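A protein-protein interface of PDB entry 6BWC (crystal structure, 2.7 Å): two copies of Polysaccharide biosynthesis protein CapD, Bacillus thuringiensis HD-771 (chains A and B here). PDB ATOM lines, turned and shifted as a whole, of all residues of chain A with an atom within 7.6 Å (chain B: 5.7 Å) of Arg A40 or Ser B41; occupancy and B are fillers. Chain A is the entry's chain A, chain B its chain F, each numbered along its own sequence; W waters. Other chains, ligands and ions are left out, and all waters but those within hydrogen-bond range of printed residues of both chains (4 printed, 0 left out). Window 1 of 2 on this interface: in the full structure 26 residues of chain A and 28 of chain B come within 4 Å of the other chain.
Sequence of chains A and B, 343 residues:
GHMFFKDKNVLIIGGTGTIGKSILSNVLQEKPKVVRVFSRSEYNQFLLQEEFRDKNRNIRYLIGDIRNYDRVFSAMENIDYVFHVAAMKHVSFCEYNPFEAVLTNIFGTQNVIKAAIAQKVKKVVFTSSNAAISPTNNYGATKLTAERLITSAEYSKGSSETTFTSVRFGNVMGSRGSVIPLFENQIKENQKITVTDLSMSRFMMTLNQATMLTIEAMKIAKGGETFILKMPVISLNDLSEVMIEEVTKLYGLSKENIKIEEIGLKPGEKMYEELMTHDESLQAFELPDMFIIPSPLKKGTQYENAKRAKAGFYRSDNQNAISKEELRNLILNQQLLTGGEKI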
ATOM      1  N   GLY A  14      13.213 -31.084 -13.346  1.00  0.00           N
ATOM      2  CA  GLY A  14      12.320 -30.618 -14.440  1.00  0.00           C
ATOM      3  C   GLY A  14      10.865 -31.055 -14.252  1.00  0.00           C
ATOM      4  O   GLY A  14      10.097 -31.221 -15.218  1.00  0.00           O
ATOM      5  N   THR A  16       8.175 -29.653 -13.097  1.00  0.00           N
ATOM      6  CA  THR A  16       7.018 -28.777 -13.357  1.00  0.00           C
ATOM      7  C   THR A  16       6.477 -28.918 -14.780  1.00  0.00           C
ATOM      8  O   THR A  16       5.328 -28.560 -15.038  1.00  0.00           O
ATOM      9  CB  THR A  16       7.305 -27.276 -13.039  1.00  0.00           C
ATOM     10  OG1 THR A  16       8.607 -26.873 -13.518  1.00  0.00           O
ATOM     11  CG2 THR A  16       7.205 -27.021 -11.532  1.00  0.00           C
ATOM     12  N   PHE A  38      12.085 -30.416  -8.696  1.00  0.00           N
ATOM     13  CA  PHE A  38      13.172 -29.425  -8.791  1.00  0.00           C
ATOM     14  C   PHE A  38      12.986 -28.634 -10.094  1.00  0.00           C
ATOM     15  O   PHE A  38      13.014 -29.197 -11.205  1.00  0.00           O
ATOM     16  CB  PHE A  38      14.519 -30.173  -8.783  1.00  0.00           C
ATOM     17  CG  PHE A  38      15.753 -29.304  -8.846  1.00  0.00           C
ATOM     18  CD1 PHE A  38      16.554 -29.138  -7.719  1.00  0.00           C
ATOM     19  CD2 PHE A  38      16.188 -28.748 -10.043  1.00  0.00           C
ATOM     20  CE1 PHE A  38      17.725 -28.407  -7.764  1.00  0.00           C
ATOM     21  CE2 PHE A  38      17.371 -28.028 -10.103  1.00  0.00           C
ATOM     22  CZ  PHE A  38      18.138 -27.862  -8.958  1.00  0.00           C
ATOM     23  N   SER A  39      12.803 -27.333  -9.967  1.00  0.00           N
ATOM     24  CA  SER A  39      12.625 -26.491 -11.141  1.00  0.00           C
ATOM     25  C   SER A  39      12.914 -25.061 -10.709  1.00  0.00           C
ATOM     26  O   SER A  39      13.034 -24.808  -9.513  1.00  0.00           O
ATOM     27  CB  SER A  39      11.202 -26.660 -11.676  1.00  0.00           C
ATOM     28  OG  SER A  39      10.217 -26.465 -10.657  1.00  0.00           O
ATOM     29  N   ARG A  40      13.049 -24.128 -11.639  1.00  0.00           N
ATOM     30  CA  ARG A  40      13.460 -22.777 -11.233  1.00  0.00           C
ATOM     31  C   ARG A  40      12.326 -21.816 -10.918  1.00  0.00           C
ATOM     32  O   ARG A  40      12.477 -20.933 -10.098  1.00  0.00           O
ATOM     33  CB  ARG A  40      14.262 -22.095 -12.319  1.00  0.00           C
ATOM     34  CG  ARG A  40      15.404 -22.884 -12.912  1.00  0.00           C
ATOM     35  CD  ARG A  40      15.698 -22.266 -14.269  1.00  0.00           C
ATOM     36  NE  ARG A  40      14.561 -22.428 -15.182  1.00  0.00           N
ATOM     37  CZ  ARG A  40      14.586 -22.103 -16.468  1.00  0.00           C
ATOM     38  NH1 ARG A  40      15.699 -21.587 -17.006  1.00  0.00           N
ATOM     39  NH2 ARG A  40      13.495 -22.300 -17.215  1.00  0.00           N
ATOM     40  N   SER A  41      11.216 -21.957 -11.615  1.00  0.00           N
ATOM     41  CA  SER A  41      10.282 -20.886 -11.747  1.00  0.00           C
ATOM     42  C   SER A  41       9.145 -21.082 -10.758  1.00  0.00           C
ATOM     43  O   SER A  41       8.423 -22.082 -10.800  1.00  0.00           O
ATOM     44  CB  SER A  41       9.833 -20.792 -13.202  1.00  0.00           C
ATOM     45  OG  SER A  41       8.422 -20.815 -13.328  1.00  0.00           O
ATOM     46  N   GLU A  42       8.998 -20.099  -9.873  1.00  0.00           N
ATOM     47  CA  GLU A  42       8.124 -20.213  -8.701  1.00  0.00           C
ATOM     48  C   GLU A  42       6.640 -20.194  -9.035  1.00  0.00           C
ATOM     49  O   GLU A  42       5.867 -20.878  -8.360  1.00  0.00           O
ATOM     50  CB  GLU A  42       8.453 -19.148  -7.642  1.00  0.00           C
ATOM     51  CG  GLU A  42       8.141 -17.734  -8.068  1.00  0.00           C
ATOM     52  CD  GLU A  42       8.672 -16.668  -7.126  1.00  0.00           C
ATOM     53  OE1 GLU A  42       8.714 -15.548  -7.658  1.00  0.00           O
ATOM     54  OE2 GLU A  42       9.004 -16.901  -5.913  1.00  0.00           O
ATOM     55  N   TYR A  43       6.238 -19.430 -10.059  1.00  0.00           N
ATOM     56  CA  TYR A  43       4.835 -19.447 -10.535  1.00  0.00           C
ATOM     57  C   TYR A  43       4.369 -20.856 -10.922  1.00  0.00           C
ATOM     58  O   TYR A  43       3.241 -21.260 -10.597  1.00  0.00           O
ATOM     59  CB  TYR A  43       4.660 -18.508 -11.728  1.00  0.00           C
ATOM     60  CG  TYR A  43       3.320 -18.592 -12.412  1.00  0.00           C
ATOM     61  CD1 TYR A  43       2.137 -18.383 -11.702  1.00  0.00           C
ATOM     62  CD2 TYR A  43       3.224 -18.872 -13.782  1.00  0.00           C
ATOM     63  CE1 TYR A  43       0.898 -18.449 -12.329  1.00  0.00           C
ATOM     64  CE2 TYR A  43       1.981 -18.942 -14.424  1.00  0.00           C
ATOM     65  CZ  TYR A  43       0.826 -18.733 -13.687  1.00  0.00           C
ATOM     66  OH  TYR A  43      -0.393 -18.806 -14.311  1.00  0.00           O
ATOM     67  N   ASN A  44       5.245 -21.596 -11.610  1.00  0.00           N
ATOM     68  CA  ASN A  44       4.941 -22.957 -12.043  1.00  0.00           C
ATOM     69  C   ASN A  44       4.919 -23.960 -10.870  1.00  0.00           C
ATOM     70  O   ASN A  44       4.014 -24.812 -10.787  1.00  0.00           O
ATOM     71  CB  ASN A  44       5.935 -23.419 -13.118  1.00  0.00           C
ATOM     72  CG  ASN A  44       5.657 -22.830 -14.500  1.00  0.00           C
ATOM     73  OD1 ASN A  44       4.622 -22.205 -14.757  1.00  0.00           O
ATOM     74  ND2 ASN A  44       6.594 -23.059 -15.413  1.00  0.00           N
ATOM     75  N   GLN A  45       5.899 -23.885  -9.965  1.00  0.00           N
ATOM     76  CA  GLN A  45       5.816 -24.700  -8.746  1.00  0.00           C
ATOM     77  C   GLN A  45       4.562 -24.377  -7.948  1.00  0.00           C
ATOM     78  O   GLN A  45       4.011 -25.250  -7.296  1.00  0.00           O
ATOM     79  CB  GLN A  45       7.040 -24.532  -7.856  1.00  0.00           C
ATOM     80  CG  GLN A  45       8.256 -25.216  -8.446  1.00  0.00           C
ATOM     81  CD  GLN A  45       9.340 -25.551  -7.454  1.00  0.00           C
ATOM     82  OE1 GLN A  45       9.245 -25.278  -6.275  1.00  0.00           O
ATOM     83  NE2 GLN A  45      10.397 -26.141  -7.956  1.00  0.00           N
ATOM     84  N   LEU A  62      11.411 -27.960  -4.614  1.00  0.00           N
ATOM     85  CA  LEU A  62      12.699 -27.226  -4.537  1.00  0.00           C
ATOM     86  C   LEU A  62      12.871 -26.346  -5.783  1.00  0.00           C
ATOM     87  O   LEU A  62      12.714 -26.806  -6.941  1.00  0.00           O
ATOM     88  CB  LEU A  62      13.923 -28.173  -4.429  1.00  0.00           C
ATOM     89  CG  LEU A  62      14.172 -29.026  -3.168  1.00  0.00           C
ATOM     90  CD1 LEU A  62      12.991 -29.932  -2.887  1.00  0.00           C
ATOM     91  CD2 LEU A  62      15.391 -29.922  -3.298  1.00  0.00           C
ATOM     92  N   ILE A  63      13.208 -25.086  -5.533  1.00  0.00           N
ATOM     93  CA  ILE A  63      13.567 -24.139  -6.574  1.00  0.00           C
ATOM     94  C   ILE A  63      15.090 -24.212  -6.769  1.00  0.00           C
ATOM     95  O   ILE A  63      15.843 -24.104  -5.809  1.00  0.00           O
ATOM     96  CB  ILE A  63      13.138 -22.702  -6.190  1.00  0.00           C
ATOM     97  CG1 ILE A  63      11.621 -22.620  -5.903  1.00  0.00           C
ATOM     98  CG2 ILE A  63      13.552 -21.717  -7.270  1.00  0.00           C
ATOM     99  CD1 ILE A  63      10.738 -22.603  -7.129  1.00  0.00           C
ATOM    100  N   GLY A  64      15.538 -24.408  -8.002  1.00  0.00           N
ATOM    101  CA  GLY A  64      16.969 -24.579  -8.293  1.00  0.00           C
ATOM    102  C   GLY A  64      17.297 -24.642  -9.785  1.00  0.00           C
ATOM    103  O   GLY A  64      16.456 -24.998 -10.621  1.00  0.00           O
ATOM    104  N   ASP A  65      18.528 -24.286 -10.126  1.00  0.00           N
ATOM    105  CA  ASP A  65      18.943 -24.290 -11.505  1.00  0.00           C
ATOM    106  C   ASP A  65      19.998 -25.364 -11.653  1.00  0.00           C
ATOM    107  O   ASP A  65      20.982 -25.354 -10.920  1.00  0.00           O
ATOM    108  CB  ASP A  65      19.499 -22.929 -11.903  1.00  0.00           C
ATOM    109  CG  ASP A  65      19.525 -22.730 -13.413  1.00  0.00           C
ATOM    110  OD1 ASP A  65      20.209 -23.505 -14.111  1.00  0.00           O
ATOM    111  OD2 ASP A  65      18.861 -21.797 -13.912  1.00  0.00           O
ATOM    112  N   ILE A  66      19.821 -26.265 -12.622  1.00  0.00           N
ATOM    113  CA  ILE A  66      20.814 -27.304 -12.859  1.00  0.00           C
ATOM    114  C   ILE A  66      22.183 -26.751 -13.203  1.00  0.00           C
ATOM    115  O   ILE A  66      23.156 -27.492 -13.109  1.00  0.00           O
ATOM    116  CB  ILE A  66      20.398 -28.355 -13.920  1.00  0.00           C
ATOM    117  CG1 ILE A  66      20.118 -27.745 -15.293  1.00  0.00           C
ATOM    118  CG2 ILE A  66      19.199 -29.170 -13.447  1.00  0.00           C
ATOM    119  CD1 ILE A  66      20.065 -28.825 -16.369  1.00  0.00           C
ATOM    120  N   ARG A  67      22.259 -25.471 -13.598  1.00  0.00           N
ATOM    121  CA  ARG A  67      23.547 -24.790 -13.841  1.00  0.00           C
ATOM    122  C   ARG A  67      24.370 -24.573 -12.539  1.00  0.00           C
ATOM    123  O   ARG A  67      25.608 -24.399 -12.574  1.00  0.00           O
ATOM    124  CB  ARG A  67      23.324 -23.456 -14.561  1.00  0.00           C
ATOM    125  CG  ARG A  67      22.661 -23.545 -15.937  1.00  0.00           C
ATOM    126  CD  ARG A  67      22.238 -22.141 -16.391  1.00  0.00           C
ATOM    127  NE  ARG A  67      21.400 -22.109 -17.608  1.00  0.00           N
ATOM    128  CZ  ARG A  67      21.283 -21.068 -18.442  1.00  0.00           C
ATOM    129  NH1 ARG A  67      21.964 -19.929 -18.249  1.00  0.00           N
ATOM    130  NH2 ARG A  67      20.487 -21.165 -19.501  1.00  0.00           N
ATOM    131  N   ALA A  86      15.146 -31.766 -17.189  1.00  0.00           N
ATOM    132  CA  ALA A  86      15.305 -30.348 -17.497  1.00  0.00           C
ATOM    133  C   ALA A  86      16.244 -30.124 -18.672  1.00  0.00           C
ATOM    134  O   ALA A  86      17.354 -30.685 -18.725  1.00  0.00           O
ATOM    135  CB  ALA A  86      15.812 -29.605 -16.282  1.00  0.00           C
ATOM    136  N   ALA A  87      15.787 -29.309 -19.620  1.00  0.00           N
ATOM    137  CA  ALA A  87      16.652 -28.790 -20.705  1.00  0.00           C
ATOM    138  C   ALA A  87      16.049 -27.518 -21.354  1.00  0.00           C
ATOM    139  O   ALA A  87      14.984 -27.054 -20.937  1.00  0.00           O
ATOM    140  CB  ALA A  87      16.888 -29.870 -21.758  1.00  0.00           C
ATOM    141  N   MET A  88      16.738 -26.946 -22.337  1.00  0.00           N
ATOM    142  CA  MET A  88      16.100 -26.066 -23.315  1.00  0.00           C
ATOM    143  C   MET A  88      15.764 -26.964 -24.481  1.00  0.00           C
ATOM    144  O   MET A  88      16.659 -27.595 -25.032  1.00  0.00           O
ATOM    145  CB  MET A  88      17.049 -24.972 -23.810  1.00  0.00           C
ATOM    146  CG  MET A  88      17.348 -23.873 -22.809  1.00  0.00           C
ATOM    147  SD  MET A  88      18.302 -22.459 -23.448  1.00  0.00           S
ATOM    148  CE  MET A  88      17.959 -21.460 -22.014  1.00  0.00           C
ATOM    149  N   HIS A  90      13.474 -25.994 -27.346  1.00  0.00           N
ATOM    150  CA  HIS A  90      13.122 -25.388 -28.629  1.00  0.00           C
ATOM    151  C   HIS A  90      14.398 -25.328 -29.501  1.00  0.00           C
ATOM    152  O   HIS A  90      15.487 -25.008 -29.021  1.00  0.00           O
ATOM    153  CB  HIS A  90      12.521 -24.002 -28.454  1.00  0.00           C
ATOM    154  CG  HIS A  90      11.106 -23.986 -27.951  1.00  0.00           C
ATOM    155  ND1 HIS A  90      10.788 -24.031 -26.613  1.00  0.00           N
ATOM    156  CD2 HIS A  90       9.930 -23.841 -28.602  1.00  0.00           C
ATOM    157  CE1 HIS A  90       9.477 -23.962 -26.459  1.00  0.00           C
ATOM    158  NE2 HIS A  90       8.932 -23.838 -27.653  1.00  0.00           N
ATOM    159  N   PHE A  93      15.181 -21.507 -30.242  1.00  0.00           N
ATOM    160  CA  PHE A  93      15.781 -20.821 -29.097  1.00  0.00           C
ATOM    161  C   PHE A  93      17.248 -21.180 -28.842  1.00  0.00           C
ATOM    162  O   PHE A  93      18.065 -20.298 -28.544  1.00  0.00           O
ATOM    163  CB  PHE A  93      14.945 -21.034 -27.849  1.00  0.00           C
ATOM    164  CG  PHE A  93      13.782 -20.094 -27.751  1.00  0.00           C
ATOM    165  CD1 PHE A  93      13.971 -18.779 -27.347  1.00  0.00           C
ATOM    166  CD2 PHE A  93      12.497 -20.502 -28.069  1.00  0.00           C
ATOM    167  CE1 PHE A  93      12.897 -17.902 -27.242  1.00  0.00           C
ATOM    168  CE2 PHE A  93      11.419 -19.626 -27.963  1.00  0.00           C
ATOM    169  CZ  PHE A  93      11.620 -18.324 -27.549  1.00  0.00           C
ATOM    170  N   GLU A 100      23.410 -20.289 -23.892  1.00  0.00           N
ATOM    171  CA  GLU A 100      22.402 -20.625 -22.868  1.00  0.00           C
ATOM    172  C   GLU A 100      21.959 -22.075 -22.918  1.00  0.00           C
ATOM    173  O   GLU A 100      21.626 -22.668 -21.898  1.00  0.00           O
ATOM    174  CB  GLU A 100      21.160 -19.777 -23.062  1.00  0.00           C
ATOM    175  CG  GLU A 100      21.347 -18.319 -22.753  1.00  0.00           C
ATOM    176  CD  GLU A 100      21.618 -18.090 -21.303  1.00  0.00           C
ATOM    177  OE1 GLU A 100      20.810 -18.547 -20.462  1.00  0.00           O
ATOM    178  OE2 GLU A 100      22.655 -17.481 -21.021  1.00  0.00           O
ATOM    179  N   THR A 104      22.450 -25.049 -19.900  1.00  0.00           N
ATOM    180  CA  THR A 104      21.430 -25.914 -19.322  1.00  0.00           C
ATOM    181  C   THR A 104      21.640 -27.354 -19.790  1.00  0.00           C
ATOM    182  O   THR A 104      21.548 -28.272 -18.982  1.00  0.00           O
ATOM    183  CB  THR A 104      19.999 -25.439 -19.664  1.00  0.00           C
ATOM    184  OG1 THR A 104      19.700 -24.169 -19.067  1.00  0.00           O
ATOM    185  CG2 THR A 104      18.984 -26.397 -19.126  1.00  0.00           C
ATOM    186  N   ARG A 176       4.307 -28.515 -23.830  1.00  0.00           N
ATOM    187  CA  ARG A 176       4.492 -27.058 -23.669  1.00  0.00           C
ATOM    188  C   ARG A 176       5.274 -26.324 -24.770  1.00  0.00           C
ATOM    189  O   ARG A 176       6.478 -26.524 -24.940  1.00  0.00           O
ATOM    190  CB  ARG A 176       5.175 -26.765 -22.332  1.00  0.00           C
ATOM    191  CG  ARG A 176       4.219 -26.565 -21.169  1.00  0.00           C
ATOM    192  CD  ARG A 176       4.917 -26.617 -19.804  1.00  0.00           C
ATOM    193  NE  ARG A 176       6.375 -26.362 -19.824  1.00  0.00           N
ATOM    194  CZ  ARG A 176       7.008 -25.309 -19.283  1.00  0.00           C
ATOM    195  NH1 ARG A 176       6.357 -24.323 -18.660  1.00  0.00           N
ATOM    196  NH2 ARG A 176       8.333 -25.230 -19.366  1.00  0.00           N
ATOM    197  N   THR B  16       8.910 -10.843 -19.590  1.00  0.00           N
ATOM    198  CA  THR B  16       7.864 -11.846 -19.878  1.00  0.00           C
ATOM    199  C   THR B  16       6.706 -11.799 -18.880  1.00  0.00           C
ATOM    200  O   THR B  16       5.577 -12.213 -19.225  1.00  0.00           O
ATOM    201  CB  THR B  16       8.429 -13.288 -19.881  1.00  0.00           C
ATOM    202  OG1 THR B  16       9.354 -13.438 -18.787  1.00  0.00           O
ATOM    203  CG2 THR B  16       9.114 -13.620 -21.236  1.00  0.00           C
ATOM    204  N   SER B  39      14.803 -12.849 -20.024  1.00  0.00           N
ATOM    205  CA  SER B  39      14.009 -13.740 -19.197  1.00  0.00           C
ATOM    206  C   SER B  39      14.561 -15.169 -19.323  1.00  0.00           C
ATOM    207  O   SER B  39      15.172 -15.499 -20.325  1.00  0.00           O
ATOM    208  CB  SER B  39      12.536 -13.574 -19.627  1.00  0.00           C
ATOM    209  OG  SER B  39      11.775 -14.749 -19.495  1.00  0.00           O
ATOM    210  N   ARG B  40      14.381 -16.005 -18.308  1.00  0.00           N
ATOM    211  CA  ARG B  40      14.979 -17.359 -18.324  1.00  0.00           C
ATOM    212  C   ARG B  40      14.280 -18.454 -19.143  1.00  0.00           C
ATOM    213  O   ARG B  40      14.942 -19.399 -19.582  1.00  0.00           O
ATOM    214  CB  ARG B  40      15.047 -17.922 -16.923  1.00  0.00           C
ATOM    215  CG  ARG B  40      15.863 -17.095 -15.960  1.00  0.00           C
ATOM    216  CD  ARG B  40      15.687 -17.719 -14.590  1.00  0.00           C
ATOM    217  NE  ARG B  40      14.277 -17.703 -14.219  1.00  0.00           N
ATOM    218  CZ  ARG B  40      13.800 -18.184 -13.086  1.00  0.00           C
ATOM    219  NH1 ARG B  40      14.628 -18.735 -12.192  1.00  0.00           N
ATOM    220  NH2 ARG B  40      12.482 -18.110 -12.867  1.00  0.00           N
ATOM    221  N   SER B  41      12.960 -18.355 -19.291  1.00  0.00           N
ATOM    222  CA  SER B  41      12.143 -19.516 -19.611  1.00  0.00           C
ATOM    223  C   SER B  41      11.602 -19.425 -21.026  1.00  0.00           C
ATOM    224  O   SER B  41      10.824 -18.535 -21.357  1.00  0.00           O
ATOM    225  CB  SER B  41      11.044 -19.704 -18.555  1.00  0.00           C
ATOM    226  OG  SER B  41       9.771 -19.964 -19.133  1.00  0.00           O
ATOM    227  N   GLU B  42      12.034 -20.368 -21.855  1.00  0.00           N
ATOM    228  CA  GLU B  42      11.772 -20.305 -23.287  1.00  0.00           C
ATOM    229  C   GLU B  42      10.284 -20.444 -23.602  1.00  0.00           C
ATOM    230  O   GLU B  42       9.847 -19.903 -24.600  1.00  0.00           O
ATOM    231  CB  GLU B  42      12.644 -21.316 -24.068  1.00  0.00           C
ATOM    232  CG  GLU B  42      12.325 -22.777 -23.771  1.00  0.00           C
ATOM    233  CD  GLU B  42      13.314 -23.805 -24.336  1.00  0.00           C
ATOM    234  OE1 GLU B  42      13.147 -24.963 -23.899  1.00  0.00           O
ATOM    235  OE2 GLU B  42      14.192 -23.517 -25.204  1.00  0.00           O
ATOM    236  N   TYR B  43       9.503 -21.120 -22.757  1.00  0.00           N
ATOM    237  CA  TYR B  43       8.044 -21.272 -23.002  1.00  0.00           C
ATOM    238  C   TYR B  43       7.327 -19.925 -22.996  1.00  0.00           C
ATOM    239  O   TYR B  43       6.514 -19.626 -23.874  1.00  0.00           O
ATOM    240  CB  TYR B  43       7.390 -22.212 -21.961  1.00  0.00           C
ATOM    241  CG  TYR B  43       5.871 -22.298 -22.054  1.00  0.00           C
ATOM    242  CD1 TYR B  43       5.257 -22.719 -23.240  1.00  0.00           C
ATOM    243  CD2 TYR B  43       5.042 -21.957 -20.967  1.00  0.00           C
ATOM    244  CE1 TYR B  43       3.880 -22.788 -23.359  1.00  0.00           C
ATOM    245  CE2 TYR B  43       3.645 -22.026 -21.079  1.00  0.00           C
ATOM    246  CZ  TYR B  43       3.078 -22.443 -22.287  1.00  0.00           C
ATOM    247  OH  TYR B  43       1.707 -22.541 -22.462  1.00  0.00           O
ATOM    248  N   ASN B  44       7.650 -19.129 -21.981  1.00  0.00           N
ATOM    249  CA  ASN B  44       7.150 -17.772 -21.850  1.00  0.00           C
ATOM    250  C   ASN B  44       7.652 -16.833 -22.953  1.00  0.00           C
ATOM    251  O   ASN B  44       6.885 -16.000 -23.446  1.00  0.00           O
ATOM    252  CB  ASN B  44       7.519 -17.193 -20.479  1.00  0.00           C
ATOM    253  CG  ASN B  44       6.745 -17.831 -19.344  1.00  0.00           C
ATOM    254  OD1 ASN B  44       5.618 -18.290 -19.523  1.00  0.00           O
ATOM    255  ND2 ASN B  44       7.340 -17.846 -18.163  1.00  0.00           N
ATOM    256  N   GLN B  45       8.927 -16.929 -23.332  1.00  0.00           N
ATOM    257  CA  GLN B  45       9.407 -16.105 -24.444  1.00  0.00           C
ATOM    258  C   GLN B  45       8.657 -16.502 -25.720  1.00  0.00           C
ATOM    259  O   GLN B  45       8.267 -15.654 -26.508  1.00  0.00           O
ATOM    260  CB  GLN B  45      10.928 -16.201 -24.624  1.00  0.00           C
ATOM    261  CG  GLN B  45      11.697 -15.628 -23.432  1.00  0.00           C
ATOM    262  CD  GLN B  45      13.015 -14.960 -23.787  1.00  0.00           C
ATOM    263  OE1 GLN B  45      13.505 -15.070 -24.900  1.00  0.00           O
ATOM    264  NE2 GLN B  45      13.593 -14.282 -22.825  1.00  0.00           N
ATOM    265  N   PHE B  46       8.430 -17.796 -25.893  1.00  0.00           N
ATOM    266  CA  PHE B  46       7.718 -18.294 -27.055  1.00  0.00           C
ATOM    267  C   PHE B  46       6.318 -17.660 -27.072  1.00  0.00           C
ATOM    268  O   PHE B  46       5.942 -17.008 -28.051  1.00  0.00           O
ATOM    269  CB  PHE B  46       7.671 -19.845 -27.008  1.00  0.00           C
ATOM    270  CG  PHE B  46       6.918 -20.487 -28.148  1.00  0.00           C
ATOM    271  CD1 PHE B  46       7.444 -20.471 -29.449  1.00  0.00           C
ATOM    272  CD2 PHE B  46       5.685 -21.135 -27.918  1.00  0.00           C
ATOM    273  CE1 PHE B  46       6.748 -21.071 -30.496  1.00  0.00           C
ATOM    274  CE2 PHE B  46       4.987 -21.732 -28.959  1.00  0.00           C
ATOM    275  CZ  PHE B  46       5.519 -21.702 -30.244  1.00  0.00           C
ATOM    276  N   ILE B  63      17.162 -14.934 -23.890  1.00  0.00           N
ATOM    277  CA  ILE B  63      17.097 -15.873 -22.776  1.00  0.00           C
ATOM    278  C   ILE B  63      18.366 -15.747 -21.920  1.00  0.00           C
ATOM    279  O   ILE B  63      19.470 -15.764 -22.448  1.00  0.00           O
ATOM    280  CB  ILE B  63      17.004 -17.325 -23.256  1.00  0.00           C
ATOM    281  CG1 ILE B  63      15.754 -17.545 -24.115  1.00  0.00           C
ATOM    282  CG2 ILE B  63      17.000 -18.257 -22.058  1.00  0.00           C
ATOM    283  CD1 ILE B  63      14.482 -17.773 -23.334  1.00  0.00           C
ATOM    284  N   ASP B  65      19.868 -15.302 -17.382  1.00  0.00           N
ATOM    285  CA  ASP B  65      19.622 -15.305 -15.953  1.00  0.00           C
ATOM    286  C   ASP B  65      20.387 -14.195 -15.247  1.00  0.00           C
ATOM    287  O   ASP B  65      21.604 -14.153 -15.305  1.00  0.00           O
ATOM    288  CB  ASP B  65      20.028 -16.649 -15.381  1.00  0.00           C
ATOM    289  CG  ASP B  65      19.381 -16.919 -14.073  1.00  0.00           C
ATOM    290  OD1 ASP B  65      19.467 -16.054 -13.163  1.00  0.00           O
ATOM    291  OD2 ASP B  65      18.768 -17.995 -13.951  1.00  0.00           O
ATOM    292  N   MET B  88      12.359 -13.165  -7.440  1.00  0.00           N
ATOM    293  CA  MET B  88      11.415 -14.111  -6.848  1.00  0.00           C
ATOM    294  C   MET B  88      10.529 -13.266  -5.966  1.00  0.00           C
ATOM    295  O   MET B  88      11.016 -12.596  -5.059  1.00  0.00           O
ATOM    296  CB  MET B  88      12.087 -15.156  -5.959  1.00  0.00           C
ATOM    297  CG  MET B  88      12.877 -16.237  -6.649  1.00  0.00           C
ATOM    298  SD  MET B  88      13.332 -17.498  -5.438  1.00  0.00           S
ATOM    299  CE  MET B  88      14.327 -18.498  -6.512  1.00  0.00           C
HETATM  300  O   HOH W   1      18.055 -19.758 -11.844  1.00  0.00           O
HETATM  301  O   HOH W   2      18.683 -19.997 -15.896  1.00  0.00           O
HETATM  302  O   HOH W   3       4.677 -19.917 -17.383  1.00  0.00           O
HETATM  303  O   HOH W   4       7.363 -19.400 -15.444  1.00  0.00           O
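Among the printed residues, pairs that only touch across the chains: Arg A40 with Ser B41, Ser A41 with Arg B40, Glu A42 with Met B88, Ile A63 with Met B88, Asp A65 with Asp B65, Met A88 with Glu B42, Met A88 with Ile B63, His A90 with Phe B46, Phe A93 with Glu B42, Phe A93 with Gln B45, Phe A93 with Phe B46, Phe A93 with Ile B63, Glu A100 with Ile B63 and Arg A176 with Tyr B43.
Of the 12 printed residues of chain B, 9 touch a printed residue of chain A.
Hydrophobic or aromatic side chains of chain B within 4 Å of the printed part of chain A: Tyr B43, Phe B46, Ile B63 and Met B88.
Printed residues of chain A that touch a printed residue of chain B: Arg A40, Ser A41, Glu A42, Ile A63, Asp A65, Met A88, His A90, Phe A93, Glu A100 and Arg A176.
Among the printed residues, 16 pairs touch across the chains.
Water W2 lies within hydrogen-bond range of OD2 of Asp A65 (2.7 Å) and OD2 of Asp B65 (2.8 Å).
Water W4 lies within hydrogen-bond range of OG of Ser A41 (2.8 Å) and ND2 of Asn B44 (3.1 Å).
Water W1 lies within hydrogen-bond range of the side-chain carboxylate of Asp B65 and the side-chain carboxylate of Asp A65.
Water W3 bridges the side-chain amide oxygen of Asn B44 (2.8 Å) and the side-chain amide oxygen of Asn A44 (3.5 Å).
N of His A90 sits at hydrogen-bond distance from OE2 of Glu B42, at 3.4 Å.
The backbone carbonyl oxygen (O) of Arg B40 is in hydrogen-bond range of the guanidinium group (NH1) of Arg A40 (3.5 Å).
Arg A40 touches two residues of chain B.
Printed residues of chain B within 4 Å of Asp A65: Asp B65.
Printed residues of chain B within 4 Å of Met A88: Glu B42 (3.2 Å) and Ile B63 (3.3 Å).
Of chain A, only Arg A40 comes within 4 Å of Ser B41.
Printed residues of chain A within 4 Å of Phe B46: His A90 (3.9 Å) and Phe A93 (3.6 Å).
Of the printed residues of chain A, Asp B65 touches Asp A65.
The nearest printed residue of chain B that does not touch Ile A63 is Arg B40 (5.9 Å).
Arg A40 touches its own counterpart, Arg B40.
Arg A40 touches Ser B41, and with the chains exchanged Ser A41 touches Arg B40.
Glu A42 touches Met B88, and with the chains exchanged Met A88 touches Glu B42.
Ile A63 touches Met B88, and with the chains exchanged Met A88 touches Ile B63.
Of the 16 pairs that touch across the chains among the printed residues, 8 have their exchanged pair printed and touching as well.
The guanidinium group (NH2) of Arg A67 is in salt-bridge range of the side-chain carboxylate (OE1) of Glu A100 (2.8 Å).
The guanidinium group (NE) of Arg A67 lies within salt-bridge range of the side-chain carboxylate (OD1) of Asp A65, 3.9 Å away.
The side-chain amide nitrogen (ND2) of Asn A44 lies close to the guanidinium group (NH1) of Arg A176, 3.5 Å away.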
